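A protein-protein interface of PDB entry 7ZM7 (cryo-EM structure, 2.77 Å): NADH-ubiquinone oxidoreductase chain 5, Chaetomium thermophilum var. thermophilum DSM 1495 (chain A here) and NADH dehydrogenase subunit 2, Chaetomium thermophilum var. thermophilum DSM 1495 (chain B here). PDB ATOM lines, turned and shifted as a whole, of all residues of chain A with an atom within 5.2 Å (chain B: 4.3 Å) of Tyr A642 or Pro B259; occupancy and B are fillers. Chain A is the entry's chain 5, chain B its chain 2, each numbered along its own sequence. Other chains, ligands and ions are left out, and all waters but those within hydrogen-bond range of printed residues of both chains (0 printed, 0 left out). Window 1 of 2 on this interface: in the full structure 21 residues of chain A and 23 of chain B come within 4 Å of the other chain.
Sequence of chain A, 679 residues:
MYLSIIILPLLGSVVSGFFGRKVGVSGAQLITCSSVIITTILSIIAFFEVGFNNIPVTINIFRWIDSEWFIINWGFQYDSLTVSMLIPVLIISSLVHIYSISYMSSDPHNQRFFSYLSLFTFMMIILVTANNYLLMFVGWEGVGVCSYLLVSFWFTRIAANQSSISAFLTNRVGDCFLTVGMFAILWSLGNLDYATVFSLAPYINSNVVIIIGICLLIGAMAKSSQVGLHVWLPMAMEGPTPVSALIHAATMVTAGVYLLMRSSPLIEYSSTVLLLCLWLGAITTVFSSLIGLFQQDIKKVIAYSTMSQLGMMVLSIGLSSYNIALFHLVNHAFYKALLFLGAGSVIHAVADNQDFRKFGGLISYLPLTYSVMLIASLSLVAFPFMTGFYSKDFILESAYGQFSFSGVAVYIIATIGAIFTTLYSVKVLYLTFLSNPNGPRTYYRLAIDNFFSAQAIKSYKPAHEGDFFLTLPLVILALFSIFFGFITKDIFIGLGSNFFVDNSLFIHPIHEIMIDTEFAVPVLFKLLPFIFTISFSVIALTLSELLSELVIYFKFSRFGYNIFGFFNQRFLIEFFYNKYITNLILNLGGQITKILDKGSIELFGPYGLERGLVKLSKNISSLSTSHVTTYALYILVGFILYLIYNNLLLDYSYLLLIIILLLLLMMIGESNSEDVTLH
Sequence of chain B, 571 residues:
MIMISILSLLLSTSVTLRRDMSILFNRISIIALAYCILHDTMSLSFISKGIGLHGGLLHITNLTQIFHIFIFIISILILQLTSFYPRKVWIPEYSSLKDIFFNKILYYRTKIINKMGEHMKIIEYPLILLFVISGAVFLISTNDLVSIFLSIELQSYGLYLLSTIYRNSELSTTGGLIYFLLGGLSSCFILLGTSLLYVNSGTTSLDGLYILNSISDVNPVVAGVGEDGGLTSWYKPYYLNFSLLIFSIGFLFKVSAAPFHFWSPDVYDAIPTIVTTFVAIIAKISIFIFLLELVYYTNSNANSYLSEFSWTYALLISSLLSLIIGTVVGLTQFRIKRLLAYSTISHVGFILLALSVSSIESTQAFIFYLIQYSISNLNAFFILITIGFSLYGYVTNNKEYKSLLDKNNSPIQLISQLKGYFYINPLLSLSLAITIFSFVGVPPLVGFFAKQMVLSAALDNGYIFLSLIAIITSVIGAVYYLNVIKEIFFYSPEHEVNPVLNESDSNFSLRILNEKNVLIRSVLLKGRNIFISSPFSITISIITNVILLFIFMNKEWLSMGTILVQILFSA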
ATOM      1  N   GLY A 638     -31.344   2.755 -13.607  1.00  0.00           N
ATOM      2  CA  GLY A 638     -31.132   1.985 -12.394  1.00  0.00           C
ATOM      3  C   GLY A 638     -29.933   1.068 -12.472  1.00  0.00           C
ATOM      4  O   GLY A 638     -29.390   0.667 -11.446  1.00  0.00           O
ATOM      5  N   PHE A 639     -29.520   0.705 -13.682  1.00  0.00           N
ATOM      6  CA  PHE A 639     -28.276  -0.041 -13.851  1.00  0.00           C
ATOM      7  C   PHE A 639     -27.050   0.836 -13.634  1.00  0.00           C
ATOM      8  O   PHE A 639     -26.098   0.411 -12.982  1.00  0.00           O
ATOM      9  CB  PHE A 639     -28.261  -0.707 -15.220  1.00  0.00           C
ATOM     10  CG  PHE A 639     -27.141  -1.685 -15.411  1.00  0.00           C
ATOM     11  CD1 PHE A 639     -27.094  -2.861 -14.687  1.00  0.00           C
ATOM     12  CD2 PHE A 639     -26.080  -1.385 -16.253  1.00  0.00           C
ATOM     13  CE1 PHE A 639     -26.050  -3.758 -14.854  1.00  0.00           C
ATOM     14  CE2 PHE A 639     -25.047  -2.267 -16.426  1.00  0.00           C
ATOM     15  CZ  PHE A 639     -25.024  -3.451 -15.725  1.00  0.00           C
ATOM     16  N   ILE A 640     -27.055   2.059 -14.154  1.00  0.00           N
ATOM     17  CA  ILE A 640     -25.885   2.920 -14.019  1.00  0.00           C
ATOM     18  C   ILE A 640     -25.622   3.248 -12.558  1.00  0.00           C
ATOM     19  O   ILE A 640     -24.477   3.218 -12.094  1.00  0.00           O
ATOM     20  CB  ILE A 640     -26.062   4.193 -14.859  1.00  0.00           C
ATOM     21  CG1 ILE A 640     -26.256   3.837 -16.328  1.00  0.00           C
ATOM     22  CG2 ILE A 640     -24.889   5.139 -14.656  1.00  0.00           C
ATOM     23  CD1 ILE A 640     -25.089   3.101 -16.930  1.00  0.00           C
ATOM     24  N   LEU A 641     -26.677   3.557 -11.812  1.00  0.00           N
ATOM     25  CA  LEU A 641     -26.507   3.922 -10.414  1.00  0.00           C
ATOM     26  C   LEU A 641     -25.915   2.771  -9.611  1.00  0.00           C
ATOM     27  O   LEU A 641     -25.149   2.995  -8.668  1.00  0.00           O
ATOM     28  CB  LEU A 641     -27.849   4.369  -9.843  1.00  0.00           C
ATOM     29  CG  LEU A 641     -28.522   5.438 -10.700  1.00  0.00           C
ATOM     30  CD1 LEU A 641     -30.002   5.536 -10.414  1.00  0.00           C
ATOM     31  CD2 LEU A 641     -27.850   6.777 -10.467  1.00  0.00           C
ATOM     32  N   TYR A 642     -26.268   1.531  -9.957  1.00  0.00           N
ATOM     33  CA  TYR A 642     -25.674   0.387  -9.276  1.00  0.00           C
ATOM     34  C   TYR A 642     -24.193   0.270  -9.579  1.00  0.00           C
ATOM     35  O   TYR A 642     -23.395  -0.027  -8.688  1.00  0.00           O
ATOM     36  CB  TYR A 642     -26.396  -0.901  -9.662  1.00  0.00           C
ATOM     37  CG  TYR A 642     -27.617  -1.162  -8.833  1.00  0.00           C
ATOM     38  CD1 TYR A 642     -28.509  -0.153  -8.551  1.00  0.00           C
ATOM     39  CD2 TYR A 642     -27.872  -2.408  -8.325  1.00  0.00           C
ATOM     40  CE1 TYR A 642     -29.622  -0.392  -7.802  1.00  0.00           C
ATOM     41  CE2 TYR A 642     -28.986  -2.657  -7.582  1.00  0.00           C
ATOM     42  CZ  TYR A 642     -29.850  -1.653  -7.316  1.00  0.00           C
ATOM     43  OH  TYR A 642     -30.961  -1.906  -6.557  1.00  0.00           O
ATOM     44  N   LEU A 643     -23.813   0.480 -10.834  1.00  0.00           N
ATOM     45  CA  LEU A 643     -22.407   0.437 -11.210  1.00  0.00           C
ATOM     46  C   LEU A 643     -21.624   1.562 -10.560  1.00  0.00           C
ATOM     47  O   LEU A 643     -20.527   1.341 -10.041  1.00  0.00           O
ATOM     48  CB  LEU A 643     -22.273   0.492 -12.729  1.00  0.00           C
ATOM     49  CG  LEU A 643     -22.421  -0.819 -13.497  1.00  0.00           C
ATOM     50  CD1 LEU A 643     -21.293  -1.725 -13.088  1.00  0.00           C
ATOM     51  CD2 LEU A 643     -23.721  -1.506 -13.223  1.00  0.00           C
ATOM     52  N   ILE A 644     -22.173   2.773 -10.569  1.00  0.00           N
ATOM     53  CA  ILE A 644     -21.513   3.879  -9.889  1.00  0.00           C
ATOM     54  C   ILE A 644     -21.356   3.577  -8.414  1.00  0.00           C
ATOM     55  O   ILE A 644     -20.267   3.717  -7.851  1.00  0.00           O
ATOM     56  CB  ILE A 644     -22.285   5.188 -10.118  1.00  0.00           C
ATOM     57  CG1 ILE A 644     -22.112   5.654 -11.563  1.00  0.00           C
ATOM     58  CG2 ILE A 644     -21.849   6.238  -9.130  1.00  0.00           C
ATOM     59  CD1 ILE A 644     -23.016   6.792 -11.934  1.00  0.00           C
ATOM     60  N   TYR A 645     -22.425   3.120  -7.770  1.00  0.00           N
ATOM     61  CA  TYR A 645     -22.357   2.873  -6.338  1.00  0.00           C
ATOM     62  C   TYR A 645     -21.271   1.871  -5.994  1.00  0.00           C
ATOM     63  O   TYR A 645     -20.423   2.131  -5.136  1.00  0.00           O
ATOM     64  CB  TYR A 645     -23.703   2.386  -5.829  1.00  0.00           C
ATOM     65  CG  TYR A 645     -23.680   2.049  -4.369  1.00  0.00           C
ATOM     66  CD1 TYR A 645     -23.781   3.037  -3.404  1.00  0.00           C
ATOM     67  CD2 TYR A 645     -23.545   0.736  -3.953  1.00  0.00           C
ATOM     68  CE1 TYR A 645     -23.756   2.726  -2.064  1.00  0.00           C
ATOM     69  CE2 TYR A 645     -23.520   0.415  -2.623  1.00  0.00           C
ATOM     70  CZ  TYR A 645     -23.626   1.410  -1.679  1.00  0.00           C
ATOM     71  OH  TYR A 645     -23.596   1.080  -0.347  1.00  0.00           O
ATOM     72  N   ASN A 646     -21.263   0.727  -6.665  1.00  0.00           N
ATOM     73  CA  ASN A 646     -20.388  -0.365  -6.279  1.00  0.00           C
ATOM     74  C   ASN A 646     -19.159  -0.447  -7.177  1.00  0.00           C
ATOM     75  O   ASN A 646     -18.685  -1.539  -7.485  1.00  0.00           O
ATOM     76  CB  ASN A 646     -21.181  -1.669  -6.283  1.00  0.00           C
ATOM     77  CG  ASN A 646     -20.424  -2.821  -5.672  1.00  0.00           C
ATOM     78  OD1 ASN A 646     -19.286  -2.679  -5.253  1.00  0.00           O
ATOM     79  ND2 ASN A 646     -21.060  -3.974  -5.616  1.00  0.00           N
ATOM     80  N   ASN A 647     -18.673   0.672  -7.659  1.00  0.00           N
ATOM     81  CA  ASN A 647     -17.363   0.730  -8.285  1.00  0.00           C
ATOM     82  C   ASN A 647     -16.550   1.933  -7.844  1.00  0.00           C
ATOM     83  O   ASN A 647     -15.325   1.839  -7.750  1.00  0.00           O
ATOM     84  CB  ASN A 647     -17.492   0.719  -9.809  1.00  0.00           C
ATOM     85  CG  ASN A 647     -18.099  -0.561 -10.323  1.00  0.00           C
ATOM     86  OD1 ASN A 647     -17.767  -1.649  -9.858  1.00  0.00           O
ATOM     87  ND2 ASN A 647     -18.981  -0.442 -11.312  1.00  0.00           N
ATOM     88  N   ILE B 249     -28.357  -7.959 -11.721  1.00  0.00           N
ATOM     89  CA  ILE B 249     -29.281  -6.953 -12.228  1.00  0.00           C
ATOM     90  C   ILE B 249     -30.350  -7.592 -13.101  1.00  0.00           C
ATOM     91  O   ILE B 249     -31.530  -7.227 -13.028  1.00  0.00           O
ATOM     92  CB  ILE B 249     -28.510  -5.860 -12.990  1.00  0.00           C
ATOM     93  CG1 ILE B 249     -27.693  -4.992 -12.020  1.00  0.00           C
ATOM     94  CG2 ILE B 249     -29.451  -5.023 -13.790  1.00  0.00           C
ATOM     95  CD1 ILE B 249     -28.447  -4.532 -10.836  1.00  0.00           C
ATOM     96  N   LEU B 252     -32.604  -9.490 -10.763  1.00  0.00           N
ATOM     97  CA  LEU B 252     -33.433  -8.542 -10.026  1.00  0.00           C
ATOM     98  C   LEU B 252     -34.634  -8.115 -10.845  1.00  0.00           C
ATOM     99  O   LEU B 252     -35.740  -8.002 -10.316  1.00  0.00           O
ATOM    100  CB  LEU B 252     -32.620  -7.315  -9.624  1.00  0.00           C
ATOM    101  CG  LEU B 252     -31.643  -7.481  -8.463  1.00  0.00           C
ATOM    102  CD1 LEU B 252     -30.824  -6.238  -8.329  1.00  0.00           C
ATOM    103  CD2 LEU B 252     -32.321  -7.856  -7.155  1.00  0.00           C
ATOM    104  N   ALA B 257     -37.692  -6.595  -8.483  1.00  0.00           N
ATOM    105  CA  ALA B 257     -37.230  -5.831  -7.304  1.00  0.00           C
ATOM    106  C   ALA B 257     -36.924  -4.391  -7.739  1.00  0.00           C
ATOM    107  O   ALA B 257     -36.248  -4.234  -8.767  1.00  0.00           O
ATOM    108  CB  ALA B 257     -35.999  -6.493  -6.751  1.00  0.00           C
ATOM    109  N   ALA B 258     -37.383  -3.387  -6.982  1.00  0.00           N
ATOM    110  CA  ALA B 258     -37.047  -1.983  -7.294  1.00  0.00           C
ATOM    111  C   ALA B 258     -35.530  -1.811  -7.188  1.00  0.00           C
ATOM    112  O   ALA B 258     -34.945  -2.362  -6.261  1.00  0.00           O
ATOM    113  CB  ALA B 258     -37.763  -1.084  -6.326  1.00  0.00           C
ATOM    114  N   PRO B 259     -34.864  -1.061  -8.092  1.00  0.00           N
ATOM    115  CA  PRO B 259     -35.556  -0.152  -9.020  1.00  0.00           C
ATOM    116  C   PRO B 259     -36.203  -0.723 -10.295  1.00  0.00           C
ATOM    117  O   PRO B 259     -36.968  -0.018 -10.885  1.00  0.00           O
ATOM    118  CB  PRO B 259     -34.428   0.833  -9.344  1.00  0.00           C
ATOM    119  CG  PRO B 259     -33.190  -0.016  -9.352  1.00  0.00           C
ATOM    120  CD  PRO B 259     -33.416  -1.017  -8.241  1.00  0.00           C
ATOM    121  N   PHE B 260     -35.884  -1.958 -10.685  1.00  0.00           N
ATOM    122  CA  PHE B 260     -36.371  -2.564 -11.956  1.00  0.00           C
ATOM    123  C   PHE B 260     -37.717  -3.238 -11.739  1.00  0.00           C
ATOM    124  O   PHE B 260     -37.800  -4.450 -11.948  1.00  0.00           O
ATOM    125  CB  PHE B 260     -35.320  -3.570 -12.421  1.00  0.00           C
ATOM    126  CG  PHE B 260     -33.903  -3.174 -12.094  1.00  0.00           C
ATOM    127  CD1 PHE B 260     -33.191  -2.333 -12.933  1.00  0.00           C
ATOM    128  CD2 PHE B 260     -33.283  -3.636 -10.944  1.00  0.00           C
ATOM    129  CE1 PHE B 260     -31.892  -1.964 -12.630  1.00  0.00           C
ATOM    130  CE2 PHE B 260     -31.985  -3.259 -10.641  1.00  0.00           C
ATOM    131  CZ  PHE B 260     -31.292  -2.424 -11.482  1.00  0.00           C
ATOM    132  N   HIS B 261     -38.741  -2.469 -11.391  1.00  0.00           N
ATOM    133  CA  HIS B 261     -40.045  -3.066 -11.006  1.00  0.00           C
ATOM    134  C   HIS B 261     -41.216  -2.488 -11.795  1.00  0.00           C
ATOM    135  O   HIS B 261     -42.308  -3.019 -11.642  1.00  0.00           O
ATOM    136  CB  HIS B 261     -40.285  -2.740  -9.524  1.00  0.00           C
ATOM    137  CG  HIS B 261     -40.644  -1.310  -9.306  1.00  0.00           C
ATOM    138  ND1 HIS B 261     -39.710  -0.299  -9.372  1.00  0.00           N
ATOM    139  CD2 HIS B 261     -41.830  -0.711  -9.068  1.00  0.00           C
ATOM    140  CE1 HIS B 261     -40.301   0.857  -9.174  1.00  0.00           C
ATOM    141  NE2 HIS B 261     -41.599   0.631  -8.992  1.00  0.00           N
ATOM    142  N   PHE B 262     -41.020  -1.477 -12.628  1.00  0.00           N
ATOM    143  CA  PHE B 262     -42.174  -0.771 -13.248  1.00  0.00           C
ATOM    144  C   PHE B 262     -42.963  -1.734 -14.141  1.00  0.00           C
ATOM    145  O   PHE B 262     -44.180  -1.537 -14.311  1.00  0.00           O
ATOM    146  CB  PHE B 262     -41.711   0.488 -13.990  1.00  0.00           C
ATOM    147  CG  PHE B 262     -41.040   1.538 -13.143  1.00  0.00           C
ATOM    148  CD1 PHE B 262     -39.670   1.517 -12.940  1.00  0.00           C
ATOM    149  CD2 PHE B 262     -41.772   2.563 -12.566  1.00  0.00           C
ATOM    150  CE1 PHE B 262     -39.051   2.489 -12.173  1.00  0.00           C
ATOM    151  CE2 PHE B 262     -41.152   3.533 -11.795  1.00  0.00           C
ATOM    152  CZ  PHE B 262     -39.793   3.495 -11.600  1.00  0.00           C
ATOM    153  N   ALA B 314     -25.970  -4.831  -4.057  1.00  0.00           N
ATOM    154  CA  ALA B 314     -27.080  -4.522  -4.975  1.00  0.00           C
ATOM    155  C   ALA B 314     -28.381  -5.111  -4.422  1.00  0.00           C
ATOM    156  O   ALA B 314     -29.416  -4.468  -4.595  1.00  0.00           O
ATOM    157  CB  ALA B 314     -26.757  -5.071  -6.337  1.00  0.00           C
ATOM    158  N   ILE B 317     -29.472  -2.906  -1.516  1.00  0.00           N
ATOM    159  CA  ILE B 317     -30.041  -1.616  -1.992  1.00  0.00           C
ATOM    160  C   ILE B 317     -31.386  -1.951  -2.635  1.00  0.00           C
ATOM    161  O   ILE B 317     -32.321  -1.202  -2.428  1.00  0.00           O
ATOM    162  CB  ILE B 317     -29.094  -0.896  -2.972  1.00  0.00           C
ATOM    163  CG1 ILE B 317     -27.680  -0.743  -2.420  1.00  0.00           C
ATOM    164  CG2 ILE B 317     -29.667   0.443  -3.407  1.00  0.00           C
ATOM    165  CD1 ILE B 317     -26.676  -0.482  -3.503  1.00  0.00           C
ATOM    166  N   SER B 318     -31.468  -3.069  -3.351  1.00  0.00           N
ATOM    167  CA  SER B 318     -32.757  -3.450  -3.912  1.00  0.00           C
ATOM    168  C   SER B 318     -33.772  -3.704  -2.823  1.00  0.00           C
ATOM    169  O   SER B 318     -34.919  -3.262  -2.923  1.00  0.00           O
ATOM    170  CB  SER B 318     -32.628  -4.687  -4.794  1.00  0.00           C
ATOM    171  OG  SER B 318     -32.186  -4.347  -6.083  1.00  0.00           O
ATOM    172  N   LEU B 321     -34.877  -0.419  -1.346  1.00  0.00           N
ATOM    173  CA  LEU B 321     -35.740   0.299  -2.273  1.00  0.00           C
ATOM    174  C   LEU B 321     -37.062  -0.420  -2.485  1.00  0.00           C
ATOM    175  O   LEU B 321     -38.089   0.221  -2.709  1.00  0.00           O
ATOM    176  CB  LEU B 321     -35.023   0.496  -3.605  1.00  0.00           C
ATOM    177  CG  LEU B 321     -33.851   1.469  -3.622  1.00  0.00           C
ATOM    178  CD1 LEU B 321     -33.356   1.638  -5.028  1.00  0.00           C
ATOM    179  CD2 LEU B 321     -34.238   2.816  -3.026  1.00  0.00           C
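OG of Ser B318 lies close to O of Ala B258 (3.4 Å).
The side-chain hydroxyl (OG) of Ser B318 sits at hydrogen-bond distance from the backbone carbonyl oxygen (O) of Ala B314, 3.1 Å away.
The backbone carbonyl oxygen of Pro B259 is in hydrogen-bond range of a ring nitrogen (ND1) of His B261, at 3.1 Å.
The side-chain hydroxyl (OG) of Ser B318 is in hydrogen-bond range of the side-chain hydroxyl (OH) of Tyr A642.
Of the 12 printed residues of chain B, 6 touch a printed residue of chain A.
Printed residues of chain B that touch a printed residue of chain A: Ile B249, Pro B259, Phe B260, Ala B314, Ile B317 and Ser B318.
Hydrophobic or aromatic side chains of chain B within 4 Å of the printed part of chain A: Ile B249, Pro B259, Phe B260, Ala B314 and Ile B317.
Printed residues of chain A that touch a printed residue of chain B: Gly A638, Phe A639, Tyr A642 and Tyr A645.
Hydrophobic or aromatic side chains of chain A within 4 Å of the printed part of chain B: Phe A639, Tyr A642 and Tyr A645.
Among the printed residues, no Asp or Glu carboxylate lies within 4 Å of a Lys or Arg side-chain nitrogen of the other chain.
Among the printed residues, pairs that only touch across the chains: Gly A638 with Phe B260 (3.6 Å), Phe A639 with Ile B249 (3.3 Å), Phe A639 with Phe B260 (3.7 Å), Tyr A642 with Ile B249 (3.3 Å), Tyr A642 with Pro B259 (3.1 Å), Tyr A642 with Ala B314 (3.5 Å), Tyr A642 with Ile B317 (3.9 Å) and Tyr A645 with Ile B317 (3.4 Å).
Of the printed residues of chain B, Gly A638 touches Phe B260 (3.6 Å).
Ile A640 touches none of the printed residues of chain B.
Tyr A642 touches just these residues of chain B: Ile B249, Pro B259, Ala B314, Ile B317 and Ser B318.
Of the printed residues of chain B, Tyr A645 touches Ile B317.
Printed residues of chain A within 4 Å of Ile B249: Phe A639 and Tyr A642.
Of chain A, only Tyr A642 (3.1 Å) comes within 4 Å of Pro B259.
The nearest residue of chain A that does not touch Pro B259 is Gly A638 (4.2 Å).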
